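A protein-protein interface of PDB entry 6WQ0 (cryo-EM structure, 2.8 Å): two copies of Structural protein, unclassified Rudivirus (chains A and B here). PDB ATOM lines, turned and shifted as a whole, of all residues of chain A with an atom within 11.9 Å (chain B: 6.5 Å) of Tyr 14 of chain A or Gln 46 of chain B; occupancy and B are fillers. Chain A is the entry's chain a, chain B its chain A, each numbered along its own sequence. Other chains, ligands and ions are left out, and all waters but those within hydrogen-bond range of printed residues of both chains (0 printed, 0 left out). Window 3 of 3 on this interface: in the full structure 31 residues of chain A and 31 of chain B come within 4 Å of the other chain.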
ATOM      1  N   PRO A   7     -14.511  -1.696  -0.308  1.00  0.00           N
ATOM      2  CA  PRO A   7     -13.387  -1.569   0.629  1.00  0.00           C
ATOM      3  C   PRO A   7     -13.221  -2.818   1.482  1.00  0.00           C
ATOM      4  O   PRO A   7     -14.197  -3.416   1.932  1.00  0.00           O
ATOM      5  CB  PRO A   7     -13.768  -0.350   1.477  1.00  0.00           C
ATOM      6  CG  PRO A   7     -15.212  -0.168   1.269  1.00  0.00           C
ATOM      7  CD  PRO A   7     -15.518  -0.647  -0.098  1.00  0.00           C
ATOM      8  N   ARG A   8     -11.969  -3.201   1.705  1.00  0.00           N
ATOM      9  CA  ARG A   8     -11.622  -4.359   2.517  1.00  0.00           C
ATOM     10  C   ARG A   8     -10.790  -3.910   3.709  1.00  0.00           C
ATOM     11  O   ARG A   8      -9.769  -3.240   3.540  1.00  0.00           O
ATOM     12  CB  ARG A   8     -10.857  -5.396   1.694  1.00  0.00           C
ATOM     13  CG  ARG A   8     -11.541  -5.808   0.403  1.00  0.00           C
ATOM     14  CD  ARG A   8     -12.625  -6.839   0.635  1.00  0.00           C
ATOM     15  NE  ARG A   8     -12.595  -7.873  -0.391  1.00  0.00           N
ATOM     16  CZ  ARG A   8     -13.559  -8.092  -1.273  1.00  0.00           C
ATOM     17  NH1 ARG A   8     -14.655  -7.359  -1.262  1.00  0.00           N
ATOM     18  NH2 ARG A   8     -13.425  -9.054  -2.163  1.00  0.00           N
ATOM     19  N   SER A   9     -11.233  -4.276   4.905  1.00  0.00           N
ATOM     20  CA  SER A   9     -10.548  -3.928   6.137  1.00  0.00           C
ATOM     21  C   SER A   9      -9.420  -4.919   6.399  1.00  0.00           C
ATOM     22  O   SER A   9      -9.175  -5.834   5.616  1.00  0.00           O
ATOM     23  CB  SER A   9     -11.535  -3.900   7.297  1.00  0.00           C
ATOM     24  OG  SER A   9     -12.216  -5.132   7.405  1.00  0.00           O
ATOM     25  N   PHE A  10      -8.722  -4.747   7.523  1.00  0.00           N
ATOM     26  CA  PHE A  10      -7.629  -5.662   7.829  1.00  0.00           C
ATOM     27  C   PHE A  10      -8.130  -7.083   8.044  1.00  0.00           C
ATOM     28  O   PHE A  10      -7.438  -8.039   7.685  1.00  0.00           O
ATOM     29  CB  PHE A  10      -6.845  -5.201   9.056  1.00  0.00           C
ATOM     30  CG  PHE A  10      -5.856  -6.219   9.528  1.00  0.00           C
ATOM     31  CD1 PHE A  10      -4.711  -6.469   8.801  1.00  0.00           C
ATOM     32  CD2 PHE A  10      -6.098  -6.971  10.658  1.00  0.00           C
ATOM     33  CE1 PHE A  10      -3.820  -7.426   9.206  1.00  0.00           C
ATOM     34  CE2 PHE A  10      -5.202  -7.927  11.064  1.00  0.00           C
ATOM     35  CZ  PHE A  10      -4.064  -8.151  10.338  1.00  0.00           C
ATOM     36  N   SER A  11      -9.315  -7.243   8.628  1.00  0.00           N
ATOM     37  CA  SER A  11      -9.851  -8.580   8.857  1.00  0.00           C
ATOM     38  C   SER A  11     -10.107  -9.308   7.547  1.00  0.00           C
ATOM     39  O   SER A  11      -9.748 -10.479   7.404  1.00  0.00           O
ATOM     40  CB  SER A  11     -11.135  -8.494   9.672  1.00  0.00           C
ATOM     41  OG  SER A  11     -10.877  -7.937  10.938  1.00  0.00           O
ATOM     42  N   GLN A  12     -10.716  -8.627   6.576  1.00  0.00           N
ATOM     43  CA  GLN A  12     -11.039  -9.271   5.310  1.00  0.00           C
ATOM     44  C   GLN A  12      -9.785  -9.552   4.495  1.00  0.00           C
ATOM     45  O   GLN A  12      -9.645 -10.638   3.917  1.00  0.00           O
ATOM     46  CB  GLN A  12     -12.013  -8.398   4.527  1.00  0.00           C
ATOM     47  CG  GLN A  12     -13.125  -7.828   5.374  1.00  0.00           C
ATOM     48  CD  GLN A  12     -14.118  -7.018   4.581  1.00  0.00           C
ATOM     49  OE1 GLN A  12     -14.316  -5.836   4.840  1.00  0.00           O
ATOM     50  NE2 GLN A  12     -14.763  -7.652   3.620  1.00  0.00           N
ATOM     51  N   ARG A  13      -8.863  -8.588   4.445  1.00  0.00           N
ATOM     52  CA  ARG A  13      -7.586  -8.798   3.772  1.00  0.00           C
ATOM     53  C   ARG A  13      -6.833  -9.971   4.373  1.00  0.00           C
ATOM     54  O   ARG A  13      -6.345 -10.845   3.650  1.00  0.00           O
ATOM     55  CB  ARG A  13      -6.733  -7.537   3.850  1.00  0.00           C
ATOM     56  CG  ARG A  13      -7.286  -6.364   3.115  1.00  0.00           C
ATOM     57  CD  ARG A  13      -6.228  -5.313   2.952  1.00  0.00           C
ATOM     58  NE  ARG A  13      -6.802  -3.983   2.829  1.00  0.00           N
ATOM     59  CZ  ARG A  13      -6.106  -2.906   2.499  1.00  0.00           C
ATOM     60  NH1 ARG A  13      -4.809  -3.005   2.263  1.00  0.00           N
ATOM     61  NH2 ARG A  13      -6.704  -1.733   2.411  1.00  0.00           N
ATOM     62  N   TYR A  14      -6.711 -10.000   5.700  1.00  0.00           N
ATOM     63  CA  TYR A  14      -5.981 -11.079   6.346  1.00  0.00           C
ATOM     64  C   TYR A  14      -6.671 -12.416   6.139  1.00  0.00           C
ATOM     65  O   TYR A  14      -6.007 -13.422   5.882  1.00  0.00           O
ATOM     66  CB  TYR A  14      -5.809 -10.795   7.837  1.00  0.00           C
ATOM     67  CG  TYR A  14      -5.167 -11.948   8.568  1.00  0.00           C
ATOM     68  CD1 TYR A  14      -3.833 -12.259   8.369  1.00  0.00           C
ATOM     69  CD2 TYR A  14      -5.898 -12.746   9.427  1.00  0.00           C
ATOM     70  CE1 TYR A  14      -3.246 -13.315   9.011  1.00  0.00           C
ATOM     71  CE2 TYR A  14      -5.318 -13.805  10.073  1.00  0.00           C
ATOM     72  CZ  TYR A  14      -3.990 -14.085   9.863  1.00  0.00           C
ATOM     73  OH  TYR A  14      -3.404 -15.144  10.510  1.00  0.00           O
ATOM     74  N   GLY A  15      -8.000 -12.452   6.241  1.00  0.00           N
ATOM     75  CA  GLY A  15      -8.708 -13.702   6.044  1.00  0.00           C
ATOM     76  C   GLY A  15      -8.508 -14.271   4.657  1.00  0.00           C
ATOM     77  O   GLY A  15      -8.188 -15.451   4.498  1.00  0.00           O
ATOM     78  N   LYS A  16      -8.666 -13.433   3.630  1.00  0.00           N
ATOM     79  CA  LYS A  16      -8.510 -13.934   2.271  1.00  0.00           C
ATOM     80  C   LYS A  16      -7.060 -14.289   1.962  1.00  0.00           C
ATOM     81  O   LYS A  16      -6.796 -15.304   1.304  1.00  0.00           O
ATOM     82  CB  LYS A  16      -9.039 -12.922   1.264  1.00  0.00           C
ATOM     83  CG  LYS A  16      -9.343 -13.552  -0.074  1.00  0.00           C
ATOM     84  CD  LYS A  16      -9.981 -12.595  -1.030  1.00  0.00           C
ATOM     85  CE  LYS A  16     -10.327 -13.289  -2.316  1.00  0.00           C
ATOM     86  NZ  LYS A  16     -10.752 -12.323  -3.344  1.00  0.00           N
ATOM     87  N   TRP A  17      -6.103 -13.479   2.422  1.00  0.00           N
ATOM     88  CA  TRP A  17      -4.701 -13.801   2.185  1.00  0.00           C
ATOM     89  C   TRP A  17      -4.314 -15.103   2.868  1.00  0.00           C
ATOM     90  O   TRP A  17      -3.588 -15.922   2.297  1.00  0.00           O
ATOM     91  CB  TRP A  17      -3.808 -12.652   2.657  1.00  0.00           C
ATOM     92  CG  TRP A  17      -2.351 -12.980   2.608  1.00  0.00           C
ATOM     93  CD1 TRP A  17      -1.493 -12.751   1.579  1.00  0.00           C
ATOM     94  CD2 TRP A  17      -1.584 -13.613   3.633  1.00  0.00           C
ATOM     95  NE1 TRP A  17      -0.245 -13.203   1.895  1.00  0.00           N
ATOM     96  CE2 TRP A  17      -0.274 -13.738   3.154  1.00  0.00           C
ATOM     97  CE3 TRP A  17      -1.880 -14.091   4.913  1.00  0.00           C
ATOM     98  CZ2 TRP A  17       0.738 -14.314   3.905  1.00  0.00           C
ATOM     99  CZ3 TRP A  17      -0.877 -14.663   5.651  1.00  0.00           C
ATOM    100  CH2 TRP A  17       0.416 -14.771   5.147  1.00  0.00           C
ATOM    101  N   ASN A  18      -4.796 -15.318   4.091  1.00  0.00           N
ATOM    102  CA  ASN A  18      -4.491 -16.545   4.807  1.00  0.00           C
ATOM    103  C   ASN A  18      -5.133 -17.750   4.139  1.00  0.00           C
ATOM    104  O   ASN A  18      -4.527 -18.823   4.076  1.00  0.00           O
ATOM    105  CB  ASN A  18      -4.957 -16.419   6.252  1.00  0.00           C
ATOM    106  CG  ASN A  18      -4.214 -17.334   7.177  1.00  0.00           C
ATOM    107  OD1 ASN A  18      -2.994 -17.378   7.167  1.00  0.00           O
ATOM    108  ND2 ASN A  18      -4.948 -18.086   7.976  1.00  0.00           N
ATOM    109  N   ALA A  19      -6.359 -17.595   3.634  1.00  0.00           N
ATOM    110  CA  ALA A  19      -7.006 -18.693   2.928  1.00  0.00           C
ATOM    111  C   ALA A  19      -6.222 -19.075   1.683  1.00  0.00           C
ATOM    112  O   ALA A  19      -5.959 -20.258   1.438  1.00  0.00           O
ATOM    113  CB  ALA A  19      -8.436 -18.309   2.565  1.00  0.00           C
ATOM    114  N   LYS A  20      -5.827 -18.081   0.888  1.00  0.00           N
ATOM    115  CA  LYS A  20      -5.086 -18.370  -0.333  1.00  0.00           C
ATOM    116  C   LYS A  20      -3.701 -18.941  -0.035  1.00  0.00           C
ATOM    117  O   LYS A  20      -3.217 -19.811  -0.767  1.00  0.00           O
ATOM    118  CB  LYS A  20      -4.986 -17.111  -1.187  1.00  0.00           C
ATOM    119  CG  LYS A  20      -6.316 -16.628  -1.719  1.00  0.00           C
ATOM    120  CD  LYS A  20      -6.971 -17.656  -2.625  1.00  0.00           C
ATOM    121  CE  LYS A  20      -6.578 -17.471  -4.072  1.00  0.00           C
ATOM    122  NZ  LYS A  20      -7.235 -16.298  -4.675  1.00  0.00           N
ATOM    123  N   PHE A  21      -3.051 -18.479   1.037  1.00  0.00           N
ATOM    124  CA  PHE A  21      -1.735 -19.003   1.395  1.00  0.00           C
ATOM    125  C   PHE A  21      -1.828 -20.442   1.889  1.00  0.00           C
ATOM    126  O   PHE A  21      -0.975 -21.274   1.571  1.00  0.00           O
ATOM    127  CB  PHE A  21      -1.088 -18.105   2.451  1.00  0.00           C
ATOM    128  CG  PHE A  21       0.386 -18.331   2.625  1.00  0.00           C
ATOM    129  CD1 PHE A  21       1.301 -17.591   1.903  1.00  0.00           C
ATOM    130  CD2 PHE A  21       0.861 -19.276   3.518  1.00  0.00           C
ATOM    131  CE1 PHE A  21       2.654 -17.798   2.061  1.00  0.00           C
ATOM    132  CE2 PHE A  21       2.211 -19.484   3.675  1.00  0.00           C
ATOM    133  CZ  PHE A  21       3.106 -18.742   2.948  1.00  0.00           C
ATOM    134  N   THR A  22      -2.855 -20.750   2.682  1.00  0.00           N
ATOM    135  CA  THR A  22      -3.074 -22.122   3.123  1.00  0.00           C
ATOM    136  C   THR A  22      -3.415 -23.032   1.953  1.00  0.00           C
ATOM    137  O   THR A  22      -3.032 -24.206   1.937  1.00  0.00           O
ATOM    138  CB  THR A  22      -4.186 -22.155   4.168  1.00  0.00           C
ATOM    139  OG1 THR A  22      -3.798 -21.366   5.295  1.00  0.00           O
ATOM    140  CG2 THR A  22      -4.468 -23.570   4.625  1.00  0.00           C
ATOM    141  N   ALA A  23      -4.147 -22.513   0.965  1.00  0.00           N
ATOM    142  CA  ALA A  23      -4.437 -23.304  -0.225  1.00  0.00           C
ATOM    143  C   ALA A  23      -3.168 -23.592  -1.015  1.00  0.00           C
ATOM    144  O   ALA A  23      -2.923 -24.734  -1.415  1.00  0.00           O
ATOM    145  CB  ALA A  23      -5.462 -22.584  -1.099  1.00  0.00           C
ATOM    146  N   ALA B  41       5.104 -16.369   8.491  1.00  0.00           N
ATOM    147  CA  ALA B  41       4.509 -15.466   7.513  1.00  0.00           C
ATOM    148  C   ALA B  41       3.221 -14.848   8.037  1.00  0.00           C
ATOM    149  O   ALA B  41       2.990 -13.644   7.864  1.00  0.00           O
ATOM    150  CB  ALA B  41       4.247 -16.214   6.210  1.00  0.00           C
ATOM    151  N   GLN B  42       2.364 -15.659   8.668  1.00  0.00           N
ATOM    152  CA  GLN B  42       1.162 -15.118   9.296  1.00  0.00           C
ATOM    153  C   GLN B  42       1.513 -14.073  10.343  1.00  0.00           C
ATOM    154  O   GLN B  42       0.853 -13.032  10.435  1.00  0.00           O
ATOM    155  CB  GLN B  42       0.345 -16.236   9.935  1.00  0.00           C
ATOM    156  CG  GLN B  42      -0.255 -17.214   8.966  1.00  0.00           C
ATOM    157  CD  GLN B  42      -0.772 -18.446   9.661  1.00  0.00           C
ATOM    158  OE1 GLN B  42      -0.888 -18.477  10.880  1.00  0.00           O
ATOM    159  NE2 GLN B  42      -1.076 -19.476   8.888  1.00  0.00           N
ATOM    160  N   GLY B  43       2.553 -14.332  11.136  1.00  0.00           N
ATOM    161  CA  GLY B  43       2.939 -13.380  12.163  1.00  0.00           C
ATOM    162  C   GLY B  43       3.470 -12.073  11.605  1.00  0.00           C
ATOM    163  O   GLY B  43       3.176 -11.001  12.135  1.00  0.00           O
ATOM    164  N   ASN B  44       4.256 -12.140  10.532  1.00  0.00           N
ATOM    165  CA  ASN B  44       4.747 -10.913   9.908  1.00  0.00           C
ATOM    166  C   ASN B  44       3.604 -10.112   9.301  1.00  0.00           C
ATOM    167  O   ASN B  44       3.565  -8.878   9.417  1.00  0.00           O
ATOM    168  CB  ASN B  44       5.791 -11.238   8.841  1.00  0.00           C
ATOM    169  CG  ASN B  44       7.075 -11.771   9.424  1.00  0.00           C
ATOM    170  OD1 ASN B  44       7.527 -11.323  10.468  1.00  0.00           O
ATOM    171  ND2 ASN B  44       7.667 -12.739   8.751  1.00  0.00           N
ATOM    172  N   PHE B  45       2.674 -10.798   8.637  1.00  0.00           N
ATOM    173  CA  PHE B  45       1.493 -10.135   8.101  1.00  0.00           C
ATOM    174  C   PHE B  45       0.723  -9.417   9.202  1.00  0.00           C
ATOM    175  O   PHE B  45       0.401  -8.228   9.084  1.00  0.00           O
ATOM    176  CB  PHE B  45       0.612 -11.168   7.395  1.00  0.00           C
ATOM    177  CG  PHE B  45      -0.385 -10.576   6.450  1.00  0.00           C
ATOM    178  CD1 PHE B  45      -0.066 -10.371   5.124  1.00  0.00           C
ATOM    179  CD2 PHE B  45      -1.646 -10.230   6.886  1.00  0.00           C
ATOM    180  CE1 PHE B  45      -0.983  -9.830   4.260  1.00  0.00           C
ATOM    181  CE2 PHE B  45      -2.565  -9.690   6.024  1.00  0.00           C
ATOM    182  CZ  PHE B  45      -2.236  -9.490   4.710  1.00  0.00           C
ATOM    183  N   GLN B  46       0.432 -10.129  10.294  1.00  0.00           N
ATOM    184  CA  GLN B  46      -0.322  -9.540  11.396  1.00  0.00           C
ATOM    185  C   GLN B  46       0.424  -8.389  12.044  1.00  0.00           C
ATOM    186  O   GLN B  46      -0.200  -7.449  12.542  1.00  0.00           O
ATOM    187  CB  GLN B  46      -0.630 -10.598  12.447  1.00  0.00           C
ATOM    188  CG  GLN B  46      -1.624 -11.644  12.024  1.00  0.00           C
ATOM    189  CD  GLN B  46      -1.642 -12.817  12.972  1.00  0.00           C
ATOM    190  OE1 GLN B  46      -0.839 -12.891  13.897  1.00  0.00           O
ATOM    191  NE2 GLN B  46      -2.556 -13.747  12.746  1.00  0.00           N
ATOM    192  N   THR B  47       1.752  -8.448  12.065  1.00  0.00           N
ATOM    193  CA  THR B  47       2.519  -7.378  12.683  1.00  0.00           C
ATOM    194  C   THR B  47       2.504  -6.121  11.827  1.00  0.00           C
ATOM    195  O   THR B  47       2.448  -5.008  12.358  1.00  0.00           O
ATOM    196  CB  THR B  47       3.951  -7.855  12.935  1.00  0.00           C
ATOM    197  OG1 THR B  47       3.936  -8.912  13.899  1.00  0.00           O
ATOM    198  CG2 THR B  47       4.828  -6.732  13.448  1.00  0.00           C
ATOM    199  N   ASN B  48       2.518  -6.268  10.503  1.00  0.00           N
ATOM    200  CA  ASN B  48       2.794  -5.115   9.654  1.00  0.00           C
ATOM    201  C   ASN B  48       1.594  -4.517   8.932  1.00  0.00           C
ATOM    202  O   ASN B  48       1.566  -3.302   8.745  1.00  0.00           O
ATOM    203  CB  ASN B  48       3.862  -5.474   8.618  1.00  0.00           C
ATOM    204  CG  ASN B  48       5.220  -5.626   9.235  1.00  0.00           C
ATOM    205  OD1 ASN B  48       5.809  -4.655   9.700  1.00  0.00           O
ATOM    206  ND2 ASN B  48       5.730  -6.848   9.253  1.00  0.00           N
ATOM    207  N   VAL B  49       0.617  -5.307   8.503  1.00  0.00           N
ATOM    208  CA  VAL B  49      -0.413  -4.791   7.597  1.00  0.00           C
ATOM    209  C   VAL B  49      -1.373  -3.784   8.241  1.00  0.00           C
ATOM    210  O   VAL B  49      -1.813  -2.853   7.545  1.00  0.00           O
ATOM    211  CB  VAL B  49      -1.180  -5.955   6.949  1.00  0.00           C
ATOM    212  CG1 VAL B  49      -2.245  -5.447   6.001  1.00  0.00           C
ATOM    213  CG2 VAL B  49      -0.214  -6.838   6.200  1.00  0.00           C
ATOM    214  N   PRO B  50      -1.739  -3.900   9.532  1.00  0.00           N
ATOM    215  CA  PRO B  50      -2.643  -2.889  10.119  1.00  0.00           C
ATOM    216  C   PRO B  50      -2.199  -1.442   9.939  1.00  0.00           C
ATOM    217  O   PRO B  50      -3.039  -0.562   9.691  1.00  0.00           O
ATOM    218  CB  PRO B  50      -2.669  -3.287  11.597  1.00  0.00           C
ATOM    219  CG  PRO B  50      -2.474  -4.728  11.590  1.00  0.00           C
ATOM    220  CD  PRO B  50      -1.583  -5.053  10.439  1.00  0.00           C
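The side-chain amide oxygen (OD1) of Asn 18 of chain A sits close to the side-chain amide nitrogen (NE2) of Gln 42 of chain B (3.3 Å).
The side-chain amide nitrogen (NE2) of Gln 46 of chain B sits at hydrogen-bond distance from the side-chain hydroxyl (OH) of Tyr 14 of chain A (2.8 Å).
The backbone carbonyl oxygen (O) of Asn 18 of chain A sits at hydrogen-bond distance from the side-chain hydroxyl (OG1) of Thr 22 of chain A, at 2.9 Å.
Among the printed residues, merely in contact across the chains: Tyr 14 of chain A with Phe 45 of chain B (3.3 Å), Phe 10 of chain A with Pro 50 of chain B (3.5 Å), Phe 10 of chain A with Val 49 of chain B (3.8 Å), Trp 17 of chain A with Phe 45 of chain B (3.8 Å), Trp 17 of chain A with Ala 41 of chain B (3.9 Å) and Tyr 14 of chain A with Gln 42 of chain B (3.9 Å).
Printed residues of chain B within 4 Å of Phe 10 of chain A: Val 49 and Pro 50.
Printed residues of chain B within 4 Å of Tyr 14 of chain A: Gln 42 (3.9 Å), Phe 45 (3.3 Å) and Gln 46 (2.8 Å).
Printed residues of chain B within 4 Å of Asn 18 of chain A: Gln 42.
Ala 19 of chain A touches none of the printed residues of chain B.
Printed residues of chain A within 4 Å of Ala 41 of chain B: Trp 17.
No residue of chain A comes within 4 Å of Gly 43 of chain B.
No residue of chain A comes within 4 Å of Asn 44 of chain B.
Phe 45 of chain B touches just these residues of chain A: Tyr 14 (3.3 Å) and Trp 17 (3.8 Å).
Of chain A, only Tyr 14 (2.8 Å) comes within 4 Å of Gln 46 of chain B.
Thr 47 of chain B touches none of the printed residues of chain A.
Asn 48 of chain B touches none of the printed residues of chain A.
Val 49 of chain B touches one residue of chain A.
The nearest residue of chain A that does not touch Gln 46 of chain B is Phe 10 of chain A (4.1 Å).
The nearest printed residue of chain B that does not touch Asn 18 of chain A is Phe 45 of chain B (6.4 Å).
Hydrophobic or aromatic side chains of chain A within 4 Å of the printed part of chain B: Phe 10, Tyr 14 and Trp 17.
Among the printed residues, 8 pairs touch across the chains.
Among the printed residues, no Asp or Glu carboxylate lies within 4 Å of a Lys or Arg side-chain nitrogen of the other chain.
No position is printed for both chains.
Of the 8 pairs that touch across the chains among the printed residues, none has its exchanged pair printed and touching as well.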
